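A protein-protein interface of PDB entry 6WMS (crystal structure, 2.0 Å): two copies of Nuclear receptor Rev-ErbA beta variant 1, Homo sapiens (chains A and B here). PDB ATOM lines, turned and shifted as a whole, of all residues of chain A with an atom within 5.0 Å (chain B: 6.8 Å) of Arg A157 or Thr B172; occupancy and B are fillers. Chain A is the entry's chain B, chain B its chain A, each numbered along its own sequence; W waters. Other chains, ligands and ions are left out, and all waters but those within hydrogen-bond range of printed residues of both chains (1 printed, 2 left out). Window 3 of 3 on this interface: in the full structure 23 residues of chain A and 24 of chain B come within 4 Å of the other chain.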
ATOM      1  N   GLU A 150       8.607  -3.880 -13.794  1.00  0.00           N
ATOM      2  CA  GLU A 150       8.933  -4.900 -12.796  1.00  0.00           C
ATOM      3  C   GLU A 150       8.988  -4.307 -11.390  1.00  0.00           C
ATOM      4  O   GLU A 150       8.568  -4.948 -10.422  1.00  0.00           O
ATOM      5  CB  GLU A 150      10.258  -5.583 -13.149  1.00  0.00           C
ATOM      6  CG  GLU A 150      10.340  -7.072 -12.732  1.00  0.00           C
ATOM      7  CD  GLU A 150       9.428  -8.021 -13.555  1.00  0.00           C
ATOM      8  OE1 GLU A 150       9.533  -8.058 -14.813  1.00  0.00           O
ATOM      9  OE2 GLU A 150       8.614  -8.748 -12.930  1.00  0.00           O
ATOM     10  N   ILE A 153       5.359  -3.778 -10.397  1.00  0.00           N
ATOM     11  CA  ILE A 153       4.724  -5.084 -10.246  1.00  0.00           C
ATOM     12  C   ILE A 153       5.183  -5.750  -8.956  1.00  0.00           C
ATOM     13  O   ILE A 153       4.387  -6.353  -8.229  1.00  0.00           O
ATOM     14  CB  ILE A 153       5.034  -5.963 -11.473  1.00  0.00           C
ATOM     15  CG1 ILE A 153       4.464  -5.333 -12.764  1.00  0.00           C
ATOM     16  CG2 ILE A 153       4.505  -7.353 -11.248  1.00  0.00           C
ATOM     17  CD1 ILE A 153       3.132  -5.901 -13.174  1.00  0.00           C
ATOM     18  N   ARG A 154       6.478  -5.659  -8.651  1.00  0.00           N
ATOM     19  CA  ARG A 154       6.973  -6.247  -7.409  1.00  0.00           C
ATOM     20  C   ARG A 154       6.330  -5.577  -6.203  1.00  0.00           C
ATOM     21  O   ARG A 154       5.856  -6.250  -5.283  1.00  0.00           O
ATOM     22  CB  ARG A 154       8.498  -6.145  -7.336  1.00  0.00           C
ATOM     23  CG  ARG A 154       9.083  -6.778  -6.071  1.00  0.00           C
ATOM     24  CD  ARG A 154      10.616  -6.738  -6.041  1.00  0.00           C
ATOM     25  NE  ARG A 154      11.213  -7.366  -7.216  1.00  0.00           N
ATOM     26  CZ  ARG A 154      11.805  -6.692  -8.198  1.00  0.00           C
ATOM     27  NH1 ARG A 154      11.877  -5.362  -8.144  1.00  0.00           N
ATOM     28  NH2 ARG A 154      12.324  -7.344  -9.232  1.00  0.00           N
ATOM     29  N   ALA A 155       6.287  -4.245  -6.201  1.00  0.00           N
ATOM     30  CA  ALA A 155       5.631  -3.538  -5.103  1.00  0.00           C
ATOM     31  C   ALA A 155       4.156  -3.901  -4.993  1.00  0.00           C
ATOM     32  O   ALA A 155       3.612  -3.952  -3.883  1.00  0.00           O
ATOM     33  CB  ALA A 155       5.774  -2.032  -5.277  1.00  0.00           C
ATOM     34  N   LEU A 156       3.479  -4.135  -6.123  1.00  0.00           N
ATOM     35  CA  LEU A 156       2.072  -4.504  -6.031  1.00  0.00           C
ATOM     36  C   LEU A 156       1.914  -5.887  -5.415  1.00  0.00           C
ATOM     37  O   LEU A 156       1.049  -6.091  -4.558  1.00  0.00           O
ATOM     38  CB  LEU A 156       1.410  -4.430  -7.409  1.00  0.00           C
ATOM     39  CG  LEU A 156      -0.091  -4.727  -7.477  1.00  0.00           C
ATOM     40  CD1 LEU A 156      -0.884  -3.729  -6.653  1.00  0.00           C
ATOM     41  CD2 LEU A 156      -0.539  -4.716  -8.946  1.00  0.00           C
ATOM     42  N   ARG A 157       2.738  -6.851  -5.845  1.00  0.00           N
ATOM     43  CA  ARG A 157       2.685  -8.195  -5.276  1.00  0.00           C
ATOM     44  C   ARG A 157       2.859  -8.156  -3.761  1.00  0.00           C
ATOM     45  O   ARG A 157       2.105  -8.793  -3.018  1.00  0.00           O
ATOM     46  CB  ARG A 157       3.760  -9.084  -5.916  1.00  0.00           C
ATOM     47  CG  ARG A 157       3.670 -10.556  -5.514  1.00  0.00           C
ATOM     48  CD  ARG A 157       4.850 -11.379  -6.041  1.00  0.00           C
ATOM     49  NE  ARG A 157       5.147 -11.093  -7.444  1.00  0.00           N
ATOM     50  CZ  ARG A 157       6.374 -11.087  -7.961  1.00  0.00           C
ATOM     51  NH1 ARG A 157       7.425 -11.351  -7.191  1.00  0.00           N
ATOM     52  NH2 ARG A 157       6.551 -10.809  -9.246  1.00  0.00           N
ATOM     53  N   THR A 158       3.845  -7.392  -3.289  1.00  0.00           N
ATOM     54  CA  THR A 158       4.078  -7.288  -1.853  1.00  0.00           C
ATOM     55  C   THR A 158       2.890  -6.650  -1.136  1.00  0.00           C
ATOM     56  O   THR A 158       2.455  -7.138  -0.083  1.00  0.00           O
ATOM     57  CB  THR A 158       5.355  -6.483  -1.614  1.00  0.00           C
ATOM     58  OG1 THR A 158       6.411  -7.061  -2.389  1.00  0.00           O
ATOM     59  CG2 THR A 158       5.739  -6.501  -0.140  1.00  0.00           C
ATOM     60  N   LEU A 159       2.355  -5.558  -1.683  1.00  0.00           N
ATOM     61  CA  LEU A 159       1.199  -4.909  -1.068  1.00  0.00           C
ATOM     62  C   LEU A 159      -0.005  -5.851  -1.015  1.00  0.00           C
ATOM     63  O   LEU A 159      -0.682  -5.949   0.016  1.00  0.00           O
ATOM     64  CB  LEU A 159       0.856  -3.626  -1.827  1.00  0.00           C
ATOM     65  CG  LEU A 159      -0.264  -2.780  -1.218  1.00  0.00           C
ATOM     66  CD1 LEU A 159       0.102  -2.308   0.178  1.00  0.00           C
ATOM     67  CD2 LEU A 159      -0.588  -1.607  -2.108  1.00  0.00           C
ATOM     68  N   ILE A 160      -0.276  -6.569  -2.113  1.00  0.00           N
ATOM     69  CA  ILE A 160      -1.418  -7.487  -2.145  1.00  0.00           C
ATOM     70  C   ILE A 160      -1.248  -8.594  -1.104  1.00  0.00           C
ATOM     71  O   ILE A 160      -2.115  -8.807  -0.247  1.00  0.00           O
ATOM     72  CB  ILE A 160      -1.613  -8.072  -3.558  1.00  0.00           C
ATOM     73  CG1 ILE A 160      -2.005  -6.983  -4.570  1.00  0.00           C
ATOM     74  CG2 ILE A 160      -2.658  -9.188  -3.534  1.00  0.00           C
ATOM     75  CD1 ILE A 160      -3.090  -6.028  -4.076  1.00  0.00           C
ATOM     76  N   MET A 161      -0.126  -9.314  -1.162  1.00  0.00           N
ATOM     77  CA  MET A 161       0.082 -10.424  -0.237  1.00  0.00           C
ATOM     78  C   MET A 161       0.145  -9.952   1.211  1.00  0.00           C
ATOM     79  O   MET A 161      -0.214 -10.702   2.124  1.00  0.00           O
ATOM     80  CB  MET A 161       1.354 -11.177  -0.610  1.00  0.00           C
ATOM     81  CG  MET A 161       1.225 -11.938  -1.913  1.00  0.00           C
ATOM     82  SD  MET A 161       2.741 -12.783  -2.392  1.00  0.00           S
ATOM     83  CE  MET A 161       3.926 -12.068  -1.246  1.00  0.00           C
ATOM     84  N   LYS A 162       0.591  -8.719   1.436  1.00  0.00           N
ATOM     85  CA  LYS A 162       0.542  -8.146   2.777  1.00  0.00           C
ATOM     86  C   LYS A 162      -0.896  -7.950   3.238  1.00  0.00           C
ATOM     87  O   LYS A 162      -1.224  -8.228   4.398  1.00  0.00           O
ATOM     88  CB  LYS A 162       1.300  -6.818   2.798  1.00  0.00           C
ATOM     89  CG  LYS A 162       1.087  -5.975   4.043  1.00  0.00           C
ATOM     90  CD  LYS A 162       2.077  -4.820   4.077  1.00  0.00           C
ATOM     91  CE  LYS A 162       1.454  -3.570   4.665  1.00  0.00           C
ATOM     92  NZ  LYS A 162       1.284  -3.694   6.144  1.00  0.00           N
ATOM     93  N   PHE A 171      -3.603 -11.585  -6.602  1.00  0.00           N
ATOM     94  CA  PHE A 171      -2.537 -11.054  -7.437  1.00  0.00           C
ATOM     95  C   PHE A 171      -2.603 -11.642  -8.838  1.00  0.00           C
ATOM     96  O   PHE A 171      -2.472 -10.914  -9.824  1.00  0.00           O
ATOM     97  CB  PHE A 171      -1.168 -11.319  -6.815  1.00  0.00           C
ATOM     98  CG  PHE A 171      -0.032 -10.788  -7.648  1.00  0.00           C
ATOM     99  CD1 PHE A 171       0.221  -9.427  -7.701  1.00  0.00           C
ATOM    100  CD2 PHE A 171       0.756 -11.646  -8.401  1.00  0.00           C
ATOM    101  CE1 PHE A 171       1.257  -8.928  -8.485  1.00  0.00           C
ATOM    102  CE2 PHE A 171       1.799 -11.152  -9.188  1.00  0.00           C
ATOM    103  CZ  PHE A 171       2.055  -9.808  -9.222  1.00  0.00           C
ATOM    104  N   LEU A 175      -3.247  -9.655 -12.447  1.00  0.00           N
ATOM    105  CA  LEU A 175      -2.427  -9.785 -13.649  1.00  0.00           C
ATOM    106  C   LEU A 175      -3.296 -10.162 -14.847  1.00  0.00           C
ATOM    107  O   LEU A 175      -3.065  -9.695 -15.969  1.00  0.00           O
ATOM    108  CB  LEU A 175      -1.320 -10.822 -13.429  1.00  0.00           C
ATOM    109  CG  LEU A 175      -0.104 -10.525 -12.522  1.00  0.00           C
ATOM    110  CD1 LEU A 175       0.699 -11.807 -12.321  1.00  0.00           C
ATOM    111  CD2 LEU A 175       0.827  -9.416 -13.055  1.00  0.00           C
ATOM    112  N   ARG B 157       0.416 -22.529 -12.417  1.00  0.00           N
ATOM    113  CA  ARG B 157       1.081 -21.923 -11.268  1.00  0.00           C
ATOM    114  C   ARG B 157       1.753 -22.980 -10.391  1.00  0.00           C
ATOM    115  O   ARG B 157       2.886 -22.797  -9.928  1.00  0.00           O
ATOM    116  CB  ARG B 157       0.067 -21.120 -10.455  1.00  0.00           C
ATOM    117  CG  ARG B 157       0.557 -20.760  -9.081  1.00  0.00           C
ATOM    118  CD  ARG B 157       1.233 -19.398  -9.060  1.00  0.00           C
ATOM    119  NE  ARG B 157       2.094 -19.267  -7.879  1.00  0.00           N
ATOM    120  CZ  ARG B 157       2.801 -18.184  -7.556  1.00  0.00           C
ATOM    121  NH1 ARG B 157       2.769 -17.108  -8.329  1.00  0.00           N
ATOM    122  NH2 ARG B 157       3.543 -18.182  -6.452  1.00  0.00           N
ATOM    123  N   ILE B 160       4.873 -24.336 -12.259  1.00  0.00           N
ATOM    124  CA  ILE B 160       6.006 -23.416 -12.169  1.00  0.00           C
ATOM    125  C   ILE B 160       6.572 -23.400 -10.752  1.00  0.00           C
ATOM    126  O   ILE B 160       7.795 -23.388 -10.554  1.00  0.00           O
ATOM    127  CB  ILE B 160       5.591 -22.004 -12.620  1.00  0.00           C
ATOM    128  CG1 ILE B 160       5.190 -22.008 -14.116  1.00  0.00           C
ATOM    129  CG2 ILE B 160       6.718 -21.006 -12.329  1.00  0.00           C
ATOM    130  CD1 ILE B 160       6.215 -22.653 -15.013  1.00  0.00           C
ATOM    131  N   GLU B 167      10.107 -18.906  -8.382  1.00  0.00           N
ATOM    132  CA  GLU B 167       8.889 -19.296  -9.093  1.00  0.00           C
ATOM    133  C   GLU B 167       7.883 -18.148  -9.222  1.00  0.00           C
ATOM    134  O   GLU B 167       7.325 -17.913 -10.302  1.00  0.00           O
ATOM    135  CB  GLU B 167       8.256 -20.499  -8.389  1.00  0.00           C
ATOM    136  CG  GLU B 167       7.740 -20.265  -6.938  1.00  0.00           C
ATOM    137  CD  GLU B 167       6.302 -19.767  -6.865  1.00  0.00           C
ATOM    138  OE1 GLU B 167       5.552 -19.902  -7.853  1.00  0.00           O
ATOM    139  OE2 GLU B 167       5.947 -19.159  -5.830  1.00  0.00           O
ATOM    140  N   ALA B 168       7.653 -17.403  -8.140  1.00  0.00           N
ATOM    141  CA  ALA B 168       6.669 -16.328  -8.201  1.00  0.00           C
ATOM    142  C   ALA B 168       7.032 -15.313  -9.278  1.00  0.00           C
ATOM    143  O   ALA B 168       6.153 -14.797  -9.979  1.00  0.00           O
ATOM    144  CB  ALA B 168       6.534 -15.644  -6.841  1.00  0.00           C
ATOM    145  N   SER B 169       8.325 -15.056  -9.467  1.00  0.00           N
ATOM    146  CA  SER B 169       8.729 -14.071 -10.460  1.00  0.00           C
ATOM    147  C   SER B 169       8.625 -14.643 -11.875  1.00  0.00           C
ATOM    148  O   SER B 169       8.237 -13.930 -12.813  1.00  0.00           O
ATOM    149  CB  SER B 169      10.149 -13.583 -10.164  1.00  0.00           C
ATOM    150  OG  SER B 169      10.775 -13.104 -11.344  1.00  0.00           O
ATOM    151  N   ILE B 170       8.956 -15.929 -12.047  1.00  0.00           N
ATOM    152  CA  ILE B 170       8.751 -16.593 -13.334  1.00  0.00           C
ATOM    153  C   ILE B 170       7.270 -16.585 -13.697  1.00  0.00           C
ATOM    154  O   ILE B 170       6.874 -16.200 -14.807  1.00  0.00           O
ATOM    155  CB  ILE B 170       9.309 -18.027 -13.290  1.00  0.00           C
ATOM    156  CG1 ILE B 170      10.840 -18.029 -13.097  1.00  0.00           C
ATOM    157  CG2 ILE B 170       8.946 -18.790 -14.567  1.00  0.00           C
ATOM    158  CD1 ILE B 170      11.595 -17.163 -14.085  1.00  0.00           C
ATOM    159  N   PHE B 171       6.425 -16.979 -12.747  1.00  0.00           N
ATOM    160  CA  PHE B 171       4.991 -17.005 -13.009  1.00  0.00           C
ATOM    161  C   PHE B 171       4.458 -15.614 -13.354  1.00  0.00           C
ATOM    162  O   PHE B 171       3.634 -15.468 -14.259  1.00  0.00           O
ATOM    163  CB  PHE B 171       4.238 -17.590 -11.816  1.00  0.00           C
ATOM    164  CG  PHE B 171       2.768 -17.747 -12.050  1.00  0.00           C
ATOM    165  CD1 PHE B 171       2.280 -18.772 -12.859  1.00  0.00           C
ATOM    166  CD2 PHE B 171       1.874 -16.865 -11.473  1.00  0.00           C
ATOM    167  CE1 PHE B 171       0.905 -18.919 -13.085  1.00  0.00           C
ATOM    168  CE2 PHE B 171       0.491 -16.992 -11.702  1.00  0.00           C
ATOM    169  CZ  PHE B 171       0.015 -18.027 -12.508  1.00  0.00           C
ATOM    170  N   THR B 172       4.904 -14.571 -12.642  1.00  0.00           N
ATOM    171  CA  THR B 172       4.458 -13.224 -12.972  1.00  0.00           C
ATOM    172  C   THR B 172       4.878 -12.843 -14.385  1.00  0.00           C
ATOM    173  O   THR B 172       4.080 -12.306 -15.168  1.00  0.00           O
ATOM    174  CB  THR B 172       5.012 -12.208 -11.979  1.00  0.00           C
ATOM    175  OG1 THR B 172       4.461 -12.467 -10.686  1.00  0.00           O
ATOM    176  CG2 THR B 172       4.617 -10.794 -12.399  1.00  0.00           C
ATOM    177  N   LYS B 173       6.136 -13.130 -14.728  1.00  0.00           N
ATOM    178  CA  LYS B 173       6.638 -12.812 -16.059  1.00  0.00           C
ATOM    179  C   LYS B 173       5.883 -13.580 -17.129  1.00  0.00           C
ATOM    180  O   LYS B 173       5.678 -13.068 -18.237  1.00  0.00           O
ATOM    181  CB  LYS B 173       8.137 -13.116 -16.137  1.00  0.00           C
ATOM    182  CG  LYS B 173       9.000 -12.048 -15.479  1.00  0.00           C
ATOM    183  CD  LYS B 173      10.440 -12.500 -15.436  1.00  0.00           C
ATOM    184  CE  LYS B 173      11.384 -11.400 -14.981  1.00  0.00           C
ATOM    185  NZ  LYS B 173      12.582 -12.004 -14.319  1.00  0.00           N
ATOM    186  N   LEU B 174       5.448 -14.801 -16.814  1.00  0.00           N
ATOM    187  CA  LEU B 174       4.658 -15.567 -17.772  1.00  0.00           C
ATOM    188  C   LEU B 174       3.305 -14.911 -18.010  1.00  0.00           C
ATOM    189  O   LEU B 174       2.830 -14.840 -19.152  1.00  0.00           O
ATOM    190  CB  LEU B 174       4.472 -16.995 -17.268  1.00  0.00           C
ATOM    191  CG  LEU B 174       5.224 -18.139 -17.929  1.00  0.00           C
ATOM    192  CD1 LEU B 174       4.484 -19.440 -17.628  1.00  0.00           C
ATOM    193  CD2 LEU B 174       5.384 -17.941 -19.431  1.00  0.00           C
ATOM    194  N   LEU B 175       2.665 -14.430 -16.948  1.00  0.00           N
ATOM    195  CA  LEU B 175       1.364 -13.788 -17.121  1.00  0.00           C
ATOM    196  C   LEU B 175       1.486 -12.451 -17.836  1.00  0.00           C
ATOM    197  O   LEU B 175       0.577 -12.059 -18.578  1.00  0.00           O
ATOM    198  CB  LEU B 175       0.680 -13.603 -15.766  1.00  0.00           C
ATOM    199  CG  LEU B 175      -0.368 -14.679 -15.443  1.00  0.00           C
ATOM    200  CD1 LEU B 175       0.102 -16.048 -15.898  1.00  0.00           C
ATOM    201  CD2 LEU B 175      -0.657 -14.698 -13.976  1.00  0.00           C
ATOM    202  N   LEU B 176       2.589 -11.736 -17.632  1.00  0.00           N
ATOM    203  CA  LEU B 176       2.790 -10.483 -18.350  1.00  0.00           C
ATOM    204  C   LEU B 176       2.985 -10.702 -19.845  1.00  0.00           C
ATOM    205  O   LEU B 176       2.907  -9.734 -20.596  1.00  0.00           O
ATOM    206  CB  LEU B 176       3.979  -9.716 -17.783  1.00  0.00           C
ATOM    207  CG  LEU B 176       3.724  -9.033 -16.429  1.00  0.00           C
ATOM    208  CD1 LEU B 176       5.020  -8.522 -15.842  1.00  0.00           C
ATOM    209  CD2 LEU B 176       2.745  -7.889 -16.582  1.00  0.00           C
ATOM    210  N   LYS B 177       3.237 -11.938 -20.292  1.00  0.00           N
ATOM    211  CA  LYS B 177       3.253 -12.217 -21.725  1.00  0.00           C
ATOM    212  C   LYS B 177       1.867 -12.096 -22.344  1.00  0.00           C
ATOM    213  O   LYS B 177       1.752 -11.855 -23.556  1.00  0.00           O
ATOM    214  CB  LYS B 177       3.779 -13.623 -21.996  1.00  0.00           C
ATOM    215  CG  LYS B 177       5.177 -13.877 -21.434  1.00  0.00           C
ATOM    216  CD  LYS B 177       6.227 -13.120 -22.233  1.00  0.00           C
ATOM    217  CE  LYS B 177       7.534 -13.040 -21.434  1.00  0.00           C
ATOM    218  NZ  LYS B 177       7.404 -12.019 -20.328  1.00  0.00           N
HETATM  219  O   HOH W   1       8.434 -10.591 -11.381  1.00  0.00           O
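Of the printed residues of chain A, Thr B172 touches Ile A153, Arg A157 and Phe A171.
Of the printed residues of chain A, Leu B175 touches Leu A175.
Printed residues of chain B within 4 Å of Leu A175: Leu B175 (3.6 Å).
Of the printed residues of chain A, Lys B173 touches Glu A150 (3.8 Å).
Printed residues of chain B within 4 Å of Phe A171: Thr B172 (3.3 Å).
Ile B170 touches none of the printed residues of chain A.
Of the 13 printed residues of chain A, 5 touch a printed residue of chain B.
Of the 13 printed residues of chain B, 4 touch a printed residue of chain A.
Printed residues of chain B that touch a printed residue of chain A: Thr B172, Lys B173, Leu B175 and Leu B176.
Hydrophobic or aromatic side chains of chain B within 4 Å of the printed part of chain A: Leu B175 and Leu B176.
Among the printed residues, 6 pairs touch across the chains.
OG1 of Thr B172 is in hydrogen-bond range of NH2 of Arg A157, at 3.0 Å.
The backbone carbonyl oxygen of Lys B173 lies within hydrogen-bond range of the side-chain amino group of Lys B177 (2.9 Å).
O of Ala B168 lies within hydrogen-bond range of OG1 of Thr B172 (3.0 Å).
Glu A150 touches Lys B173.
Thr B172 touches Ile A153.
Ile A153 touches Leu B176 (CD1 to CD2, 3.96 Å).
CE2 of Phe A171 touches OG1 of Thr B172, at 3.3 Å.
Leu B175 touches Leu A175 (CD2 to CD1, 3.6 Å).
Water W1 lies within hydrogen-bond range of OE2 of Glu A150 (2.4 Å), NH2 of Arg A157 (2.9 Å) and OG of Ser B169 (3.4 Å).
Leu B175 touches its own counterpart, Leu A175.
Positions printed for both chains: 157, 160, 171 and 175.
Of the 6 pairs that touch across the chains among the printed residues, 1 has its exchanged pair printed and touching as well.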
